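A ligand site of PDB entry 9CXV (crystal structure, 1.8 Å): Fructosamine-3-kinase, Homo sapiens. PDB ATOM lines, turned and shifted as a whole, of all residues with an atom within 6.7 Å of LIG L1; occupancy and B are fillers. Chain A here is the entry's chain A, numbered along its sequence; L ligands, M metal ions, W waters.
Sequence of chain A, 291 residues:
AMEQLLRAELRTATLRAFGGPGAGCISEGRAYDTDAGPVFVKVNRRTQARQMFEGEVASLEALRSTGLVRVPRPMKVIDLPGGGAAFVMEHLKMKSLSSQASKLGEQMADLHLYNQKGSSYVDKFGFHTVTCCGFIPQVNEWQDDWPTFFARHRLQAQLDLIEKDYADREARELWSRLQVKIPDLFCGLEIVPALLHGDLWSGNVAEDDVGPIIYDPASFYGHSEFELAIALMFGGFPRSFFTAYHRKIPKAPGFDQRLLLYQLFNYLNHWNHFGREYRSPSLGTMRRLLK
The side-chain amide nitrogen (ND2) of Asn 204 lies close to the indole nitrogen (NE1) of Trp 201, 3.2 Å away. O of Cys 133 lies within hydrogen-bond range of ND2 of Asn 269, 3.2 Å away. The side-chain sulfur of Cys 133 sits at hydrogen-bond distance from the side-chain carboxylate of Asp 199 (3.6 Å). The backbone carbonyl oxygen (O) of Gly 198 lies within hydrogen-bond range of the side-chain sulfur (SG) of Cys 133 (3.8 Å). A ring nitrogen (NE2) of His 273 lies within hydrogen-bond range of the backbone NH of Phe 135. The side-chain amide nitrogen (ND2) of Asn 204 sits at hydrogen-bond distance from the backbone carbonyl oxygen (O) of Asp 199. The backbone carbonyl oxygen (O) of Asn 269 is in hydrogen-bond range of a ring nitrogen (ND1) of His 273. A ring nitrogen (ND1) of His 270 lies within hydrogen-bond range of the backbone carbonyl oxygen of Asn 266, 2.9 Å away.
O4 of LIG L1 sits close to NE2 of His 270, 3.0 Å away. OD1 of Asp 199 is in hydrogen-bond range of O5 of LIG L1 (2.7 Å).
Water W2 lies within hydrogen-bond range of O6 of LIG L1 (2.9 Å), NE1 of Trp 201 (3.2 Å) and O1 of LG2 L2 (3.3 Å). Water W1 lies within hydrogen-bond range of the side-chain amide oxygen of Asn 266 (2.7 Å), the side-chain amide nitrogen of Asn 269 (2.9 Å), an oxygen (O5) of LIG L1 (3.0 Å) and a ring nitrogen (ND1) of His 270 (3.3 Å).
Merely in contact with LIG L1: Cys 133, Gly 134, Trp 201, Ile 230, Phe 234, Asn 269, His 273 and Phe 274. Hydrophobic or aromatic side chains within 4 Å of LIG L1: Trp 201, Ile 230, Phe 234, His 270, His 273 and Phe 274.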
ATOM      1  N   CYS A 133      -0.788  18.215  22.870  1.00  0.00           N
ATOM      2  CA  CYS A 133       0.109  18.979  23.759  1.00  0.00           C
ATOM      3  C   CYS A 133      -0.380  20.429  23.787  1.00  0.00           C
ATOM      4  O   CYS A 133       0.133  21.302  23.075  1.00  0.00           O
ATOM      5  CB  CYS A 133       1.589  18.876  23.346  1.00  0.00           C
ATOM      6  SG  CYS A 133       2.742  19.563  24.646  1.00  0.00           S
ATOM      7  N   GLY A 134      -1.369  20.688  24.643  1.00  0.00           N
ATOM      8  CA  GLY A 134      -2.188  21.897  24.530  1.00  0.00           C
ATOM      9  C   GLY A 134      -3.408  21.635  23.645  1.00  0.00           C
ATOM     10  O   GLY A 134      -4.182  20.710  23.905  1.00  0.00           O
ATOM     11  N   PHE A 135      -3.537  22.404  22.595  1.00  0.00           N
ATOM     12  CA  PHE A 135      -4.728  22.357  21.766  1.00  0.00           C
ATOM     13  C   PHE A 135      -4.524  21.643  20.432  1.00  0.00           C
ATOM     14  O   PHE A 135      -5.509  21.189  19.853  1.00  0.00           O
ATOM     15  CB  PHE A 135      -5.217  23.817  21.520  1.00  0.00           C
ATOM     16  CG  PHE A 135      -6.466  23.917  20.704  1.00  0.00           C
ATOM     17  CD1 PHE A 135      -7.718  23.691  21.278  1.00  0.00           C
ATOM     18  CD2 PHE A 135      -6.398  24.245  19.343  1.00  0.00           C
ATOM     19  CE1 PHE A 135      -8.909  23.797  20.518  1.00  0.00           C
ATOM     20  CE2 PHE A 135      -7.582  24.364  18.556  1.00  0.00           C
ATOM     21  CZ  PHE A 135      -8.841  24.137  19.141  1.00  0.00           C
ATOM     22  N   ILE A 136      -3.295  21.512  19.946  1.00  0.00           N
ATOM     23  CA  ILE A 136      -3.035  20.994  18.601  1.00  0.00           C
ATOM     24  C   ILE A 136      -2.941  19.469  18.693  1.00  0.00           C
ATOM     25  O   ILE A 136      -2.097  18.959  19.450  1.00  0.00           O
ATOM     26  CB  ILE A 136      -1.722  21.553  18.025  1.00  0.00           C
ATOM     27  CG1 ILE A 136      -1.881  22.968  17.450  1.00  0.00           C
ATOM     28  CG2 ILE A 136      -1.166  20.631  16.884  1.00  0.00           C
ATOM     29  CD1 ILE A 136      -0.533  23.727  17.416  1.00  0.00           C
ATOM     30  N   GLY A 198       4.256  14.115  29.183  1.00  0.00           N
ATOM     31  CA  GLY A 198       4.228  14.723  27.851  1.00  0.00           C
ATOM     32  C   GLY A 198       4.088  16.248  27.863  1.00  0.00           C
ATOM     33  O   GLY A 198       4.301  16.884  26.810  1.00  0.00           O
ATOM     34  N   ASP A 199       3.754  16.832  29.016  1.00  0.00           N
ATOM     35  CA  ASP A 199       3.598  18.270  29.072  1.00  0.00           C
ATOM     36  C   ASP A 199       3.940  18.777  30.446  1.00  0.00           C
ATOM     37  O   ASP A 199       3.152  19.473  31.114  1.00  0.00           O
ATOM     38  CB  ASP A 199       2.170  18.641  28.677  1.00  0.00           C
ATOM     39  CG  ASP A 199       2.035  20.158  28.336  1.00  0.00           C
ATOM     40  OD1 ASP A 199       3.047  20.816  28.042  1.00  0.00           O
ATOM     41  OD2 ASP A 199       0.911  20.648  28.329  1.00  0.00           O
ATOM     42  N   TRP A 201       5.289  20.975  32.231  1.00  0.00           N
ATOM     43  CA  TRP A 201       5.789  22.251  32.696  1.00  0.00           C
ATOM     44  C   TRP A 201       5.269  22.550  34.108  1.00  0.00           C
ATOM     45  O   TRP A 201       4.410  21.837  34.653  1.00  0.00           O
ATOM     46  CB  TRP A 201       5.432  23.349  31.703  1.00  0.00           C
ATOM     47  CG  TRP A 201       4.057  23.823  31.824  1.00  0.00           C
ATOM     48  CD1 TRP A 201       2.914  23.135  31.481  1.00  0.00           C
ATOM     49  CD2 TRP A 201       3.615  25.140  32.244  1.00  0.00           C
ATOM     50  NE1 TRP A 201       1.785  23.938  31.684  1.00  0.00           N
ATOM     51  CE2 TRP A 201       2.192  25.152  32.176  1.00  0.00           C
ATOM     52  CE3 TRP A 201       4.288  26.307  32.686  1.00  0.00           C
ATOM     53  CZ2 TRP A 201       1.410  26.300  32.525  1.00  0.00           C
ATOM     54  CZ3 TRP A 201       3.506  27.420  33.033  1.00  0.00           C
ATOM     55  CH2 TRP A 201       2.101  27.404  32.943  1.00  0.00           C
ATOM     56  N   ASN A 204       1.701  22.444  35.299  1.00  0.00           N
ATOM     57  CA  ASN A 204       0.951  21.175  35.286  1.00  0.00           C
ATOM     58  C   ASN A 204       1.359  20.236  36.418  1.00  0.00           C
ATOM     59  O   ASN A 204       1.022  19.047  36.367  1.00  0.00           O
ATOM     60  CB  ASN A 204       1.134  20.486  33.934  1.00  0.00           C
ATOM     61  CG  ASN A 204       0.321  21.141  32.845  1.00  0.00           C
ATOM     62  OD1 ASN A 204      -0.630  21.874  33.159  1.00  0.00           O
ATOM     63  ND2 ASN A 204       0.685  20.908  31.601  1.00  0.00           N
ATOM     64  N   ASP A 216      -3.113  17.407  33.453  1.00  0.00           N
ATOM     65  CA  ASP A 216      -3.055  17.881  32.067  1.00  0.00           C
ATOM     66  C   ASP A 216      -1.989  17.145  31.227  1.00  0.00           C
ATOM     67  O   ASP A 216      -1.208  17.782  30.509  1.00  0.00           O
ATOM     68  CB  ASP A 216      -2.722  19.373  32.078  1.00  0.00           C
ATOM     69  CG  ASP A 216      -3.218  20.095  30.850  1.00  0.00           C
ATOM     70  OD1 ASP A 216      -3.891  19.472  29.984  1.00  0.00           O
ATOM     71  OD2 ASP A 216      -2.815  21.270  30.686  1.00  0.00           O
ATOM     72  N   ILE A 230      10.621  20.755  28.726  1.00  0.00           N
ATOM     73  CA  ILE A 230       9.688  21.846  29.031  1.00  0.00           C
ATOM     74  C   ILE A 230       9.765  22.184  30.512  1.00  0.00           C
ATOM     75  O   ILE A 230       9.580  23.343  30.897  1.00  0.00           O
ATOM     76  CB  ILE A 230       8.242  21.482  28.574  1.00  0.00           C
ATOM     77  CG1 ILE A 230       7.314  22.725  28.629  1.00  0.00           C
ATOM     78  CG2 ILE A 230       7.635  20.429  29.462  1.00  0.00           C
ATOM     79  CD1 ILE A 230       5.868  22.404  28.118  1.00  0.00           C
ATOM     80  N   PHE A 234      11.039  26.545  30.989  1.00  0.00           N
ATOM     81  CA  PHE A 234      10.176  27.589  31.588  1.00  0.00           C
ATOM     82  C   PHE A 234      10.332  27.709  33.088  1.00  0.00           C
ATOM     83  O   PHE A 234       9.609  28.474  33.721  1.00  0.00           O
ATOM     84  CB  PHE A 234       8.701  27.336  31.232  1.00  0.00           C
ATOM     85  CG  PHE A 234       8.424  27.387  29.753  1.00  0.00           C
ATOM     86  CD1 PHE A 234       8.677  28.541  29.023  1.00  0.00           C
ATOM     87  CD2 PHE A 234       7.903  26.267  29.081  1.00  0.00           C
ATOM     88  CE1 PHE A 234       8.425  28.609  27.646  1.00  0.00           C
ATOM     89  CE2 PHE A 234       7.642  26.300  27.714  1.00  0.00           C
ATOM     90  CZ  PHE A 234       7.896  27.484  26.969  1.00  0.00           C
ATOM     91  N   ASN A 266       9.272  22.391  21.762  1.00  0.00           N
ATOM     92  CA  ASN A 266       8.320  23.147  22.592  1.00  0.00           C
ATOM     93  C   ASN A 266       8.214  24.596  22.096  1.00  0.00           C
ATOM     94  O   ASN A 266       7.107  25.185  22.077  1.00  0.00           O
ATOM     95  CB  ASN A 266       8.752  23.074  24.067  1.00  0.00           C
ATOM     96  CG  ASN A 266       8.362  21.722  24.691  1.00  0.00           C
ATOM     97  OD1 ASN A 266       7.163  21.426  24.928  1.00  0.00           O
ATOM     98  ND2 ASN A 266       9.414  20.818  24.893  1.00  0.00           N
ATOM     99  N   ASN A 269       5.917  24.480  19.039  1.00  0.00           N
ATOM    100  CA  ASN A 269       4.536  24.311  19.504  1.00  0.00           C
ATOM    101  C   ASN A 269       3.977  25.607  20.061  1.00  0.00           C
ATOM    102  O   ASN A 269       2.773  25.905  19.914  1.00  0.00           O
ATOM    103  CB  ASN A 269       4.534  23.210  20.583  1.00  0.00           C
ATOM    104  CG  ASN A 269       3.143  22.771  21.001  1.00  0.00           C
ATOM    105  OD1 ASN A 269       2.266  22.576  20.168  1.00  0.00           O
ATOM    106  ND2 ASN A 269       2.945  22.601  22.321  1.00  0.00           N
ATOM    107  N   HIS A 270       4.813  26.366  20.779  1.00  0.00           N
ATOM    108  CA  HIS A 270       4.345  27.654  21.304  1.00  0.00           C
ATOM    109  C   HIS A 270       4.159  28.672  20.184  1.00  0.00           C
ATOM    110  O   HIS A 270       3.254  29.502  20.269  1.00  0.00           O
ATOM    111  CB  HIS A 270       5.324  28.187  22.366  1.00  0.00           C
ATOM    112  CG  HIS A 270       5.079  27.615  23.751  1.00  0.00           C
ATOM    113  ND1 HIS A 270       5.262  26.278  24.068  1.00  0.00           N
ATOM    114  CD2 HIS A 270       4.611  28.210  24.888  1.00  0.00           C
ATOM    115  CE1 HIS A 270       4.913  26.063  25.328  1.00  0.00           C
ATOM    116  NE2 HIS A 270       4.525  27.222  25.853  1.00  0.00           N
ATOM    117  N   HIS A 273       0.889  27.839  18.755  1.00  0.00           N
ATOM    118  CA  HIS A 273      -0.246  28.141  19.645  1.00  0.00           C
ATOM    119  C   HIS A 273      -0.446  29.636  19.849  1.00  0.00           C
ATOM    120  O   HIS A 273      -1.589  30.116  19.935  1.00  0.00           O
ATOM    121  CB  HIS A 273      -0.070  27.480  21.023  1.00  0.00           C
ATOM    122  CG  HIS A 273      -0.567  26.082  21.087  1.00  0.00           C
ATOM    123  ND1 HIS A 273       0.179  24.993  20.656  1.00  0.00           N
ATOM    124  CD2 HIS A 273      -1.755  25.567  21.508  1.00  0.00           C
ATOM    125  CE1 HIS A 273      -0.512  23.878  20.843  1.00  0.00           C
ATOM    126  NE2 HIS A 273      -1.698  24.203  21.344  1.00  0.00           N
ATOM    127  N   PHE A 274       0.644  30.376  20.003  1.00  0.00           N
ATOM    128  CA  PHE A 274       0.624  31.730  20.542  1.00  0.00           C
ATOM    129  C   PHE A 274       1.235  32.751  19.591  1.00  0.00           C
ATOM    130  O   PHE A 274       1.254  33.948  19.904  1.00  0.00           O
ATOM    131  CB  PHE A 274       1.347  31.757  21.905  1.00  0.00           C
ATOM    132  CG  PHE A 274       0.835  30.737  22.870  1.00  0.00           C
ATOM    133  CD1 PHE A 274      -0.514  30.745  23.246  1.00  0.00           C
ATOM    134  CD2 PHE A 274       1.666  29.771  23.393  1.00  0.00           C
ATOM    135  CE1 PHE A 274      -1.026  29.772  24.107  1.00  0.00           C
ATOM    136  CE2 PHE A 274       1.176  28.825  24.276  1.00  0.00           C
ATOM    137  CZ  PHE A 274      -0.188  28.812  24.635  1.00  0.00           C
ATOM    138  N   TYR A 278       7.162  33.593  19.715  1.00  0.00           N
ATOM    139  CA  TYR A 278       8.040  32.427  19.861  1.00  0.00           C
ATOM    140  C   TYR A 278       8.854  32.127  18.602  1.00  0.00           C
ATOM    141  O   TYR A 278       9.503  31.062  18.523  1.00  0.00           O
ATOM    142  CB  TYR A 278       7.211  31.230  20.251  1.00  0.00           C
ATOM    143  CG  TYR A 278       6.720  31.360  21.657  1.00  0.00           C
ATOM    144  CD1 TYR A 278       7.566  31.050  22.752  1.00  0.00           C
ATOM    145  CD2 TYR A 278       5.433  31.841  21.923  1.00  0.00           C
ATOM    146  CE1 TYR A 278       7.109  31.195  24.080  1.00  0.00           C
ATOM    147  CE2 TYR A 278       4.983  31.962  23.245  1.00  0.00           C
ATOM    148  CZ  TYR A 278       5.814  31.650  24.300  1.00  0.00           C
ATOM    149  OH  TYR A 278       5.356  31.778  25.603  1.00  0.00           O
HETATM  150  N1  LIG L   1       3.146  27.284  28.302  1.00  0.00           N
HETATM  151  C1  LIG L   1       2.650  25.886  28.673  1.00  0.00           C
HETATM  152  C2  LIG L   1       1.292  25.318  28.080  1.00  0.00           C
HETATM  153  O1  LIG L   1       0.286  26.014  27.942  1.00  0.00           O
HETATM  154  C3  LIG L   1       2.169  28.350  28.573  1.00  0.00           C
HETATM  155  C4  LIG L   1       2.730  29.775  28.198  1.00  0.00           C
HETATM  156  C5  LIG L   1       4.948  29.017  28.696  1.00  0.00           C
HETATM  157  C6  LIG L   1       4.386  27.611  29.048  1.00  0.00           C
HETATM  158  C7  LIG L   1       1.134  23.779  27.752  1.00  0.00           C
HETATM  159  C8  LIG L   1       1.808  23.393  26.372  1.00  0.00           C
HETATM  160  C9  LIG L   1       1.516  24.329  25.111  1.00  0.00           C
HETATM  161  C10 LIG L   1       0.077  24.467  24.556  1.00  0.00           C
HETATM  162  O2  LIG L   1       3.956  30.058  28.999  1.00  0.00           O
HETATM  163  O3  LIG L   1      -0.786  24.967  25.578  1.00  0.00           O
HETATM  164  O4  LIG L   1       1.944  25.654  25.474  1.00  0.00           O
HETATM  165  O5  LIG L   1       3.183  23.116  26.549  1.00  0.00           O
HETATM  166  O6  LIG L   1      -0.215  23.295  27.940  1.00  0.00           O
HETATM  167  P1  LG2 L   2      -5.677  23.709  31.051  1.00  0.00           P
HETATM  168  O1  LG2 L   2      -4.360  24.440  31.249  1.00  0.00           O
HETATM  169  O2  LG2 L   2      -5.613  22.479  30.137  1.00  0.00           O
HETATM  170  O3  LG2 L   2      -6.816  24.647  30.697  1.00  0.00           O
HETATM  171  P2  LG2 L   2      -5.169  22.324  33.590  1.00  0.00           P
HETATM  172  O4  LG2 L   2      -5.467  20.819  33.582  1.00  0.00           O
HETATM  173  O5  LG2 L   2      -3.725  22.726  33.386  1.00  0.00           O
HETATM  174  O6  LG2 L   2      -6.089  23.150  32.522  1.00  0.00           O
HETATM  175  O7  LG2 L   2      -5.643  22.968  35.008  1.00  0.00           O
HETATM  176  C1  LG2 L   2      -5.493  24.401  35.151  1.00  0.00           C
HETATM  177  C2  LG2 L   2      -5.669  24.759  36.623  1.00  0.00           C
HETATM  178  O8  LG2 L   2      -6.865  24.159  37.141  1.00  0.00           O
HETATM  179  C3  LG2 L   2      -4.551  24.132  37.428  1.00  0.00           C
HETATM  180  O9  LG2 L   2      -3.384  24.960  37.435  1.00  0.00           O
HETATM  181  C4  LG2 L   2      -5.183  23.888  38.791  1.00  0.00           C
HETATM  182  O10 LG2 L   2      -5.130  25.079  39.598  1.00  0.00           O
HETATM  183  C5  LG2 L   2      -6.644  23.627  38.443  1.00  0.00           C
HETATM  184  N1  LG2 L   2      -6.962  22.178  38.377  1.00  0.00           N
HETATM  185  C6  LG2 L   2      -6.733  21.367  37.312  1.00  0.00           C
HETATM  186  N2  LG2 L   2      -7.186  20.119  37.559  1.00  0.00           N
HETATM  187  C7  LG2 L   2      -7.670  20.106  38.826  1.00  0.00           C
HETATM  188  C8  LG2 L   2      -8.289  19.106  39.717  1.00  0.00           C
HETATM  189  N3  LG2 L   2      -8.448  17.833  39.293  1.00  0.00           N
HETATM  190  N4  LG2 L   2      -8.697  19.503  40.951  1.00  0.00           N
HETATM  191  C9  LG2 L   2      -8.553  20.784  41.343  1.00  0.00           C
HETATM  192  N5  LG2 L   2      -7.982  21.744  40.586  1.00  0.00           N
HETATM  193  C10 LG2 L   2      -7.534  21.467  39.345  1.00  0.00           C
HETATM  194 MG    MG M   1      -2.432  22.843  32.025  1.00  0.00          MG
HETATM  195  O   HOH W   1       5.095  22.968  24.274  1.00  0.00           O
HETATM  196  O   HOH W   2      -1.192  23.739  30.655  1.00  0.00           O
